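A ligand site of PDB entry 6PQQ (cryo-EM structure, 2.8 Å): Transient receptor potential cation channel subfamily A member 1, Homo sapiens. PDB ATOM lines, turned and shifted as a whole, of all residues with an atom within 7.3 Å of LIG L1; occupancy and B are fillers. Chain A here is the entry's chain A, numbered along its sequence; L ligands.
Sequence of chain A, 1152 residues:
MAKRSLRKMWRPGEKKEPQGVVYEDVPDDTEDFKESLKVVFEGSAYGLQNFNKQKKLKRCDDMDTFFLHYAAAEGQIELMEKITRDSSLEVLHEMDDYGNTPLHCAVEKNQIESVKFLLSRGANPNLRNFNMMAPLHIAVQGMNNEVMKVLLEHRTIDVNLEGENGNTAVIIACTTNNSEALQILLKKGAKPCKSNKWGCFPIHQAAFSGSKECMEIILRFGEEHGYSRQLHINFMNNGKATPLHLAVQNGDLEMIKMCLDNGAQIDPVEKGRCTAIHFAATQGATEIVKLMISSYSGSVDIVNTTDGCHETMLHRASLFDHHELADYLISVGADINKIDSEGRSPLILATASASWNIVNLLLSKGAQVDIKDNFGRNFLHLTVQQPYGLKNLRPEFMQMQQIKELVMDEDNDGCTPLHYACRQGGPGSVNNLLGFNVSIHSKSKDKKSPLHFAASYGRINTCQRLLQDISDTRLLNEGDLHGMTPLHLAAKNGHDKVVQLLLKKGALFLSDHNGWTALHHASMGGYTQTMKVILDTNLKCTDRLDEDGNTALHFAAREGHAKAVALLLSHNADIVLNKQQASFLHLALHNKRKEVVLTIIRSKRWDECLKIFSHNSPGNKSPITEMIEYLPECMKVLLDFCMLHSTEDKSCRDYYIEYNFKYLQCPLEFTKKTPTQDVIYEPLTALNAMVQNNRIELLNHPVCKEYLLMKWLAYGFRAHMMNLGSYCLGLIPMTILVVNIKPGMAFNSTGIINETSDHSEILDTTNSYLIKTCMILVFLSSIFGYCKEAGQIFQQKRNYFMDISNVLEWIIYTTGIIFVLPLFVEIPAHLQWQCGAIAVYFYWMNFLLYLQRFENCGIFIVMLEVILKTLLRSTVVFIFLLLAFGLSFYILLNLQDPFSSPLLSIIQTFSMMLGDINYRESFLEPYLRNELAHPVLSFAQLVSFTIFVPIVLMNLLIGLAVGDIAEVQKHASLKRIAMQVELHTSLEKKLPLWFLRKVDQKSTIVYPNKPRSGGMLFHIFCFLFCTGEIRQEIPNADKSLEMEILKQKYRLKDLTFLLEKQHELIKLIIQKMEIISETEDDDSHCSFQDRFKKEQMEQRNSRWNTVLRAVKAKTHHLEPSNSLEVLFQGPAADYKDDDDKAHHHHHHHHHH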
ATOM      1  N   CYS A 728     -14.152   9.172  -6.862  1.00  0.00           N
ATOM      2  CA  CYS A 728     -15.231   9.756  -6.089  1.00  0.00           C
ATOM      3  C   CYS A 728     -16.592   9.246  -6.543  1.00  0.00           C
ATOM      4  O   CYS A 728     -17.545   9.243  -5.747  1.00  0.00           O
ATOM      5  CB  CYS A 728     -15.146  11.278  -6.197  1.00  0.00           C
ATOM      6  SG  CYS A 728     -16.140  12.197  -5.043  1.00  0.00           S
ATOM      7  N   LEU A 731     -16.864   6.532  -4.391  1.00  0.00           N
ATOM      8  CA  LEU A 731     -16.827   6.957  -2.994  1.00  0.00           C
ATOM      9  C   LEU A 731     -18.196   7.410  -2.498  1.00  0.00           C
ATOM     10  O   LEU A 731     -18.693   6.917  -1.492  1.00  0.00           O
ATOM     11  CB  LEU A 731     -15.802   8.061  -2.802  1.00  0.00           C
ATOM     12  CG  LEU A 731     -15.671   8.586  -1.371  1.00  0.00           C
ATOM     13  CD1 LEU A 731     -15.225   7.469  -0.473  1.00  0.00           C
ATOM     14  CD2 LEU A 731     -14.707   9.748  -1.297  1.00  0.00           C
ATOM     15  N   ILE A 732     -18.808   8.369  -3.197  1.00  0.00           N
ATOM     16  CA  ILE A 732     -20.056   9.012  -2.748  1.00  0.00           C
ATOM     17  C   ILE A 732     -21.267   8.077  -2.594  1.00  0.00           C
ATOM     18  O   ILE A 732     -21.904   8.137  -1.526  1.00  0.00           O
ATOM     19  CB  ILE A 732     -20.390  10.217  -3.660  1.00  0.00           C
ATOM     20  CG1 ILE A 732     -19.395  11.352  -3.455  1.00  0.00           C
ATOM     21  CG2 ILE A 732     -21.790  10.733  -3.428  1.00  0.00           C
ATOM     22  CD1 ILE A 732     -19.661  12.524  -4.379  1.00  0.00           C
ATOM     23  N   PRO A 733     -21.648   7.220  -3.574  1.00  0.00           N
ATOM     24  CA  PRO A 733     -22.908   6.473  -3.401  1.00  0.00           C
ATOM     25  C   PRO A 733     -22.872   5.437  -2.289  1.00  0.00           C
ATOM     26  O   PRO A 733     -23.933   5.152  -1.732  1.00  0.00           O
ATOM     27  CB  PRO A 733     -23.104   5.788  -4.766  1.00  0.00           C
ATOM     28  CG  PRO A 733     -22.282   6.544  -5.690  1.00  0.00           C
ATOM     29  CD  PRO A 733     -21.089   6.925  -4.901  1.00  0.00           C
ATOM     30  N   THR A 735     -21.428   6.029   0.602  1.00  0.00           N
ATOM     31  CA  THR A 735     -21.705   6.839   1.790  1.00  0.00           C
ATOM     32  C   THR A 735     -23.171   7.217   1.869  1.00  0.00           C
ATOM     33  O   THR A 735     -23.748   7.229   2.962  1.00  0.00           O
ATOM     34  CB  THR A 735     -20.847   8.090   1.780  1.00  0.00           C
ATOM     35  OG1 THR A 735     -21.233   8.921   0.684  1.00  0.00           O
ATOM     36  CG2 THR A 735     -19.416   7.722   1.618  1.00  0.00           C
ATOM     37  N   ILE A 736     -23.794   7.521   0.729  1.00  0.00           N
ATOM     38  CA  ILE A 736     -25.226   7.804   0.698  1.00  0.00           C
ATOM     39  C   ILE A 736     -26.015   6.562   1.106  1.00  0.00           C
ATOM     40  O   ILE A 736     -26.961   6.634   1.912  1.00  0.00           O
ATOM     41  CB  ILE A 736     -25.642   8.305  -0.693  1.00  0.00           C
ATOM     42  CG1 ILE A 736     -25.025   9.676  -0.973  1.00  0.00           C
ATOM     43  CG2 ILE A 736     -27.139   8.390  -0.830  1.00  0.00           C
ATOM     44  CD1 ILE A 736     -25.283  10.174  -2.364  1.00  0.00           C
ATOM     45  N   VAL A 738     -25.029   4.143   2.974  1.00  0.00           N
ATOM     46  CA  VAL A 738     -24.847   3.900   4.390  1.00  0.00           C
ATOM     47  C   VAL A 738     -25.701   4.846   5.229  1.00  0.00           C
ATOM     48  O   VAL A 738     -26.442   4.417   6.122  1.00  0.00           O
ATOM     49  CB  VAL A 738     -23.361   4.003   4.760  1.00  0.00           C
ATOM     50  CG1 VAL A 738     -23.176   4.177   6.232  1.00  0.00           C
ATOM     51  CG2 VAL A 738     -22.670   2.742   4.323  1.00  0.00           C
ATOM     52  N   VAL A 739     -25.653   6.151   4.935  1.00  0.00           N
ATOM     53  CA  VAL A 739     -26.362   7.109   5.785  1.00  0.00           C
ATOM     54  C   VAL A 739     -27.864   7.090   5.571  1.00  0.00           C
ATOM     55  O   VAL A 739     -28.593   7.716   6.355  1.00  0.00           O
ATOM     56  CB  VAL A 739     -25.873   8.547   5.595  1.00  0.00           C
ATOM     57  CG1 VAL A 739     -24.386   8.645   5.916  1.00  0.00           C
ATOM     58  CG2 VAL A 739     -26.181   9.044   4.198  1.00  0.00           C
ATOM     59  N   ASN A 740     -28.373   6.405   4.536  1.00  0.00           N
ATOM     60  CA  ASN A 740     -29.828   6.280   4.439  1.00  0.00           C
ATOM     61  C   ASN A 740     -30.357   4.997   5.061  1.00  0.00           C
ATOM     62  O   ASN A 740     -31.308   5.039   5.853  1.00  0.00           O
ATOM     63  CB  ASN A 740     -30.270   6.381   2.985  1.00  0.00           C
ATOM     64  CG  ASN A 740     -30.172   7.792   2.457  1.00  0.00           C
ATOM     65  OD1 ASN A 740     -30.476   8.754   3.159  1.00  0.00           O
ATOM     66  ND2 ASN A 740     -29.774   7.921   1.203  1.00  0.00           N
ATOM     67  N   ILE A 741     -29.770   3.856   4.734  1.00  0.00           N
ATOM     68  CA  ILE A 741     -30.261   2.570   5.238  1.00  0.00           C
ATOM     69  C   ILE A 741     -29.747   2.370   6.653  1.00  0.00           C
ATOM     70  O   ILE A 741     -28.565   2.589   6.933  1.00  0.00           O
ATOM     71  CB  ILE A 741     -29.823   1.426   4.314  1.00  0.00           C
ATOM     72  CG1 ILE A 741     -30.409   1.622   2.919  1.00  0.00           C
ATOM     73  CG2 ILE A 741     -30.261   0.078   4.846  1.00  0.00           C
ATOM     74  CD1 ILE A 741     -29.876   0.645   1.899  1.00  0.00           C
ATOM     75  N   THR A 766     -39.841   3.395  -0.736  1.00  0.00           N
ATOM     76  CA  THR A 766     -39.895   4.848  -0.656  1.00  0.00           C
ATOM     77  C   THR A 766     -38.796   5.483  -1.498  1.00  0.00           C
ATOM     78  O   THR A 766     -39.070   6.277  -2.408  1.00  0.00           O
ATOM     79  CB  THR A 766     -39.783   5.305   0.798  1.00  0.00           C
ATOM     80  OG1 THR A 766     -38.510   4.893   1.325  1.00  0.00           O
ATOM     81  CG2 THR A 766     -40.889   4.680   1.635  1.00  0.00           C
ATOM     82  N   ASN A 767     -37.538   5.144  -1.220  1.00  0.00           N
ATOM     83  CA  ASN A 767     -36.391   5.648  -1.963  1.00  0.00           C
ATOM     84  C   ASN A 767     -35.657   4.504  -2.639  1.00  0.00           C
ATOM     85  O   ASN A 767     -34.424   4.437  -2.624  1.00  0.00           O
ATOM     86  CB  ASN A 767     -35.451   6.429  -1.039  1.00  0.00           C
ATOM     87  CG  ASN A 767     -36.041   7.745  -0.593  1.00  0.00           C
ATOM     88  OD1 ASN A 767     -36.651   8.462  -1.376  1.00  0.00           O
ATOM     89  ND2 ASN A 767     -35.862   8.062   0.686  1.00  0.00           N
ATOM     90  N   LEU A 770     -33.196   5.493  -5.626  1.00  0.00           N
ATOM     91  CA  LEU A 770     -31.900   6.022  -5.212  1.00  0.00           C
ATOM     92  C   LEU A 770     -30.976   4.893  -4.734  1.00  0.00           C
ATOM     93  O   LEU A 770     -29.791   4.881  -5.069  1.00  0.00           O
ATOM     94  CB  LEU A 770     -32.113   7.067  -4.123  1.00  0.00           C
ATOM     95  CG  LEU A 770     -30.954   7.912  -3.589  1.00  0.00           C
ATOM     96  CD1 LEU A 770     -31.472   9.299  -3.291  1.00  0.00           C
ATOM     97  CD2 LEU A 770     -30.381   7.321  -2.322  1.00  0.00           C
ATOM     98  N   CYS A 774     -27.511   3.847  -6.592  1.00  0.00           N
ATOM     99  CA  CYS A 774     -26.270   3.844  -5.824  1.00  0.00           C
ATOM    100  C   CYS A 774     -25.582   2.477  -5.865  1.00  0.00           C
ATOM    101  O   CYS A 774     -24.350   2.412  -6.014  1.00  0.00           O
ATOM    102  CB  CYS A 774     -26.524   4.265  -4.383  1.00  0.00           C
ATOM    103  SG  CYS A 774     -26.894   6.030  -4.182  1.00  0.00           S
ATOM    104  N   TRP A 844     -12.633   5.765   2.877  1.00  0.00           N
ATOM    105  CA  TRP A 844     -12.222   7.069   3.382  1.00  0.00           C
ATOM    106  C   TRP A 844     -10.799   7.073   3.924  1.00  0.00           C
ATOM    107  O   TRP A 844     -10.222   8.163   4.074  1.00  0.00           O
ATOM    108  CB  TRP A 844     -13.172   7.571   4.452  1.00  0.00           C
ATOM    109  CG  TRP A 844     -14.486   7.978   3.936  1.00  0.00           C
ATOM    110  CD1 TRP A 844     -15.635   7.281   4.017  1.00  0.00           C
ATOM    111  CD2 TRP A 844     -14.788   9.204   3.269  1.00  0.00           C
ATOM    112  NE1 TRP A 844     -16.657   7.986   3.431  1.00  0.00           N
ATOM    113  CE2 TRP A 844     -16.163   9.172   2.965  1.00  0.00           C
ATOM    114  CE3 TRP A 844     -14.040  10.318   2.884  1.00  0.00           C
ATOM    115  CZ2 TRP A 844     -16.794  10.205   2.292  1.00  0.00           C
ATOM    116  CZ3 TRP A 844     -14.674  11.346   2.224  1.00  0.00           C
ATOM    117  CH2 TRP A 844     -16.037  11.288   1.943  1.00  0.00           C
HETATM  118  C1  LIG L   1     -22.007  12.542  -0.165  1.00  0.00           C
HETATM  119  C2  LIG L   1     -22.946  13.445   0.705  1.00  0.00           C
HETATM  120  C3  LIG L   1     -24.433  12.980   0.868  1.00  0.00           C
HETATM  121  C4  LIG L   1     -25.085  13.122   2.280  1.00  0.00           C
HETATM  122  C5  LIG L   1     -26.653  12.968   2.339  1.00  0.00           C
HETATM  123  C6  LIG L   1     -27.237  12.116   3.528  1.00  0.00           C
HETATM  124  C7  LIG L   1     -28.768  11.891   3.410  1.00  0.00           C
HETATM  125  O1  LIG L   1     -29.328  10.938   3.878  1.00  0.00           O
HETATM  126  O2  LIG L   1     -29.517  12.861   2.736  1.00  0.00           O
HETATM  127  C8  LIG L   1     -30.718  12.407   2.055  1.00  0.00           C
HETATM  128  C9  LIG L   1     -31.147  13.443   0.931  1.00  0.00           C
HETATM  129  C10 LIG L   1     -32.509  12.969   0.249  1.00  0.00           C
HETATM  130  O3  LIG L   1     -33.386  12.565   1.251  1.00  0.00           O
HETATM  131  P1  LIG L   1     -35.070  12.232   0.955  1.00  0.00           P
HETATM  132  O4  LIG L   1     -35.090  11.569  -0.404  1.00  0.00           O
HETATM  133  O5  LIG L   1     -35.842  13.479   1.248  1.00  0.00           O
HETATM  134  O6  LIG L   1     -35.536  11.033   2.100  1.00  0.00           O
HETATM  135  O7  LIG L   1     -30.045  13.371  -0.040  1.00  0.00           O
HETATM  136  C11 LIG L   1     -29.923  12.184  -0.794  1.00  0.00           C
HETATM  137  O8  LIG L   1     -30.581  11.250  -0.547  1.00  0.00           O
HETATM  138  C12 LIG L   1     -28.867  12.180  -1.961  1.00  0.00           C
HETATM  139  C13 LIG L   1     -28.226  13.600  -2.269  1.00  0.00           C
HETATM  140  C14 LIG L   1     -26.670  13.656  -2.459  1.00  0.00           C
HETATM  141  C15 LIG L   1     -26.107  14.645  -3.525  1.00  0.00           C
HETATM  142  C16 LIG L   1     -24.676  15.240  -3.263  1.00  0.00           C
HETATM  143  C17 LIG L   1     -23.516  14.748  -4.174  1.00  0.00           C
HETATM  144  C18 LIG L   1     -22.230  15.632  -4.252  1.00  0.00           C
HETATM  145  C19 LIG L   1     -20.919  15.000  -3.814  1.00  0.00           C
HETATM  146  C1  LG2 L   2     -17.572  17.232   9.301  1.00  0.00           C
HETATM  147  C2  LG2 L   2     -18.954  16.659   8.823  1.00  0.00           C
HETATM  148  C3  LG2 L   2     -20.235  17.483   9.197  1.00  0.00           C
HETATM  149  C4  LG2 L   2     -21.480  17.340   8.250  1.00  0.00           C
HETATM  150  C5  LG2 L   2     -22.824  16.881   8.907  1.00  0.00           C
HETATM  151  C6  LG2 L   2     -24.153  17.437   8.300  1.00  0.00           C
HETATM  152  C7  LG2 L   2     -25.461  16.622   8.629  1.00  0.00           C
HETATM  153  C8  LG2 L   2     -26.794  17.451   8.764  1.00  0.00           C
HETATM  154  C9  LG2 L   2     -27.985  16.582   9.273  1.00  0.00           C
HETATM  155  O1  LG2 L   2     -28.976  17.054   9.747  1.00  0.00           O
HETATM  156  O2  LG2 L   2     -27.850  15.192   9.169  1.00  0.00           O
HETATM  157  C10 LG2 L   2     -27.567  14.657   7.854  1.00  0.00           C
HETATM  158  C11 LG2 L   2     -27.671  13.066   7.865  1.00  0.00           C
HETATM  159  C12 LG2 L   2     -28.527  12.571   9.110  1.00  0.00           C
HETATM  160  O3  LG2 L   2     -29.641  11.874   8.625  1.00  0.00           O
HETATM  161  P1  LG2 L   2     -31.264  12.397   8.921  1.00  0.00           P
HETATM  162  O4  LG2 L   2     -31.201  13.910   8.883  1.00  0.00           O
HETATM  163  O5  LG2 L   2     -31.781  11.662  10.104  1.00  0.00           O
HETATM  164  O6  LG2 L   2     -32.190  11.908   7.548  1.00  0.00           O
HETATM  165  C13 LG2 L   2     -33.554  11.627   7.684  1.00  0.00           C
HETATM  166  C14 LG2 L   2     -34.171  11.215   6.319  1.00  0.00           C
HETATM  167  N1  LG2 L   2     -35.634  10.995   6.456  1.00  0.00           N
HETATM  168  O7  LG2 L   2     -26.274  12.637   8.007  1.00  0.00           O
HETATM  169  C15 LG2 L   2     -25.359  13.088   7.026  1.00  0.00           C
HETATM  170  O8  LG2 L   2     -25.736  13.426   5.970  1.00  0.00           O
HETATM  171  C16 LG2 L   2     -23.831  13.117   7.416  1.00  0.00           C
HETATM  172  C17 LG2 L   2     -22.852  12.857   6.209  1.00  0.00           C
HETATM  173  C18 LG2 L   2     -21.718  13.914   5.960  1.00  0.00           C
HETATM  174  C19 LG2 L   2     -20.344  13.386   5.434  1.00  0.00           C
HETATM  175  C20 LG2 L   2     -19.784  14.045   4.128  1.00  0.00           C
HETATM  176  C21 LG2 L   2     -18.489  14.894   4.250  1.00  0.00           C
HETATM  177  C22 LG2 L   2     -17.560  14.988   2.989  1.00  0.00           C
HETATM  178  C23 LG2 L   2     -17.378  16.359   2.356  1.00  0.00           C
HETATM  179  C1  LG3 L   3      -5.416  23.767  -3.197  1.00  0.00           C
HETATM  180  N1  LG3 L   3      -0.813  25.341  -8.631  1.00  0.00           N
HETATM  181  P1  LG3 L   3      -3.438  23.587  -5.045  1.00  0.00           P
HETATM  182  C2  LG3 L   3      -6.541  22.705  -3.427  1.00  0.00           C
HETATM  183  C3  LG3 L   3      -7.400  22.574  -2.133  1.00  0.00           C
HETATM  184  C4  LG3 L   3      -2.303  25.654  -8.326  1.00  0.00           C
HETATM  185  O1  LG3 L   3      -4.903  24.125  -4.428  1.00  0.00           O
HETATM  186  C5  LG3 L   3      -2.666  25.485  -6.805  1.00  0.00           C
HETATM  187  O2  LG3 L   3      -3.265  24.272  -6.683  1.00  0.00           O
HETATM  188  C6  LG3 L   3      -0.459  25.814 -10.028  1.00  0.00           C
HETATM  189  O3  LG3 L   3      -3.572  22.143  -5.413  1.00  0.00           O
HETATM  190  C7  LG3 L   3       0.102  26.008  -7.619  1.00  0.00           C
HETATM  191  O4  LG3 L   3      -2.331  24.258  -4.337  1.00  0.00           O
HETATM  192  C8  LG3 L   3      -0.577  23.846  -8.580  1.00  0.00           C
HETATM  193  C9  LG3 L   3      -8.355  20.406  -1.759  1.00  0.00           C
HETATM  194  O5  LG3 L   3      -8.439  21.630  -2.356  1.00  0.00           O
HETATM  195  C10 LG3 L   3      -9.677  19.843  -1.289  1.00  0.00           C
HETATM  196  O6  LG3 L   3      -7.289  19.845  -1.645  1.00  0.00           O
HETATM  197  C11 LG3 L   3     -10.096  18.534  -2.003  1.00  0.00           C
HETATM  198  C12 LG3 L   3     -11.242  17.744  -1.315  1.00  0.00           C
HETATM  199  C13 LG3 L   3     -12.482  17.402  -2.188  1.00  0.00           C
HETATM  200  C14 LG3 L   3     -13.215  16.085  -1.804  1.00  0.00           C
HETATM  201  C15 LG3 L   3     -14.767  16.137  -1.702  1.00  0.00           C
HETATM  202  C16 LG3 L   3     -15.555  14.932  -2.269  1.00  0.00           C
HETATM  203  C17 LG3 L   3     -16.860  14.557  -1.512  1.00  0.00           C
HETATM  204  C18 LG3 L   3      -7.444  22.671  -5.706  1.00  0.00           C
HETATM  205  O7  LG3 L   3      -7.455  23.170  -4.431  1.00  0.00           O
HETATM  206  C19 LG3 L   3      -8.834  22.481  -6.316  1.00  0.00           C
HETATM  207  O8  LG3 L   3      -6.391  22.400  -6.237  1.00  0.00           O
HETATM  208  C20 LG3 L   3      -9.833  21.644  -5.478  1.00  0.00           C
HETATM  209  C21 LG3 L   3     -11.320  22.084  -5.529  1.00  0.00           C
HETATM  210  C22 LG3 L   3     -12.368  20.942  -5.537  1.00  0.00           C
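The side-chain amide oxygen (OD1) of Asn 740 sits close to an oxygen (O1) of LIG L1, at 2.6 Å.
The side-chain amide nitrogen (ND2) of Asn 767 sits at hydrogen-bond distance from an oxygen (O6) of LIG L1, at 3.3 Å.
ND2 of Asn 740 sits at hydrogen-bond distance from O of Ile 736, 3.2 Å away.
The backbone carbonyl oxygen (O) of Ile 732 sits at hydrogen-bond distance from the side-chain hydroxyl (OG1) of Thr 735 (2.4 Å).
SG of Cys 774 sits at hydrogen-bond distance from O of Leu 770 (3.2 Å).
Residues that only touch LIG L1: Ile 732, Thr 735, Ile 736, Val 739 and Leu 770.
Hydrophobic or aromatic side chains within 4 Å of LIG L1: Ile 732, Ile 736, Val 739 and Leu 770.
Within 4 Å of LIG L1: Ile 732, Thr 735, Ile 736, Val 739, Asn 740, Asn 767 and Leu 770.
The nearest printed residue that does not touch LIG L1 is Cys 728 (5.7 Å).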
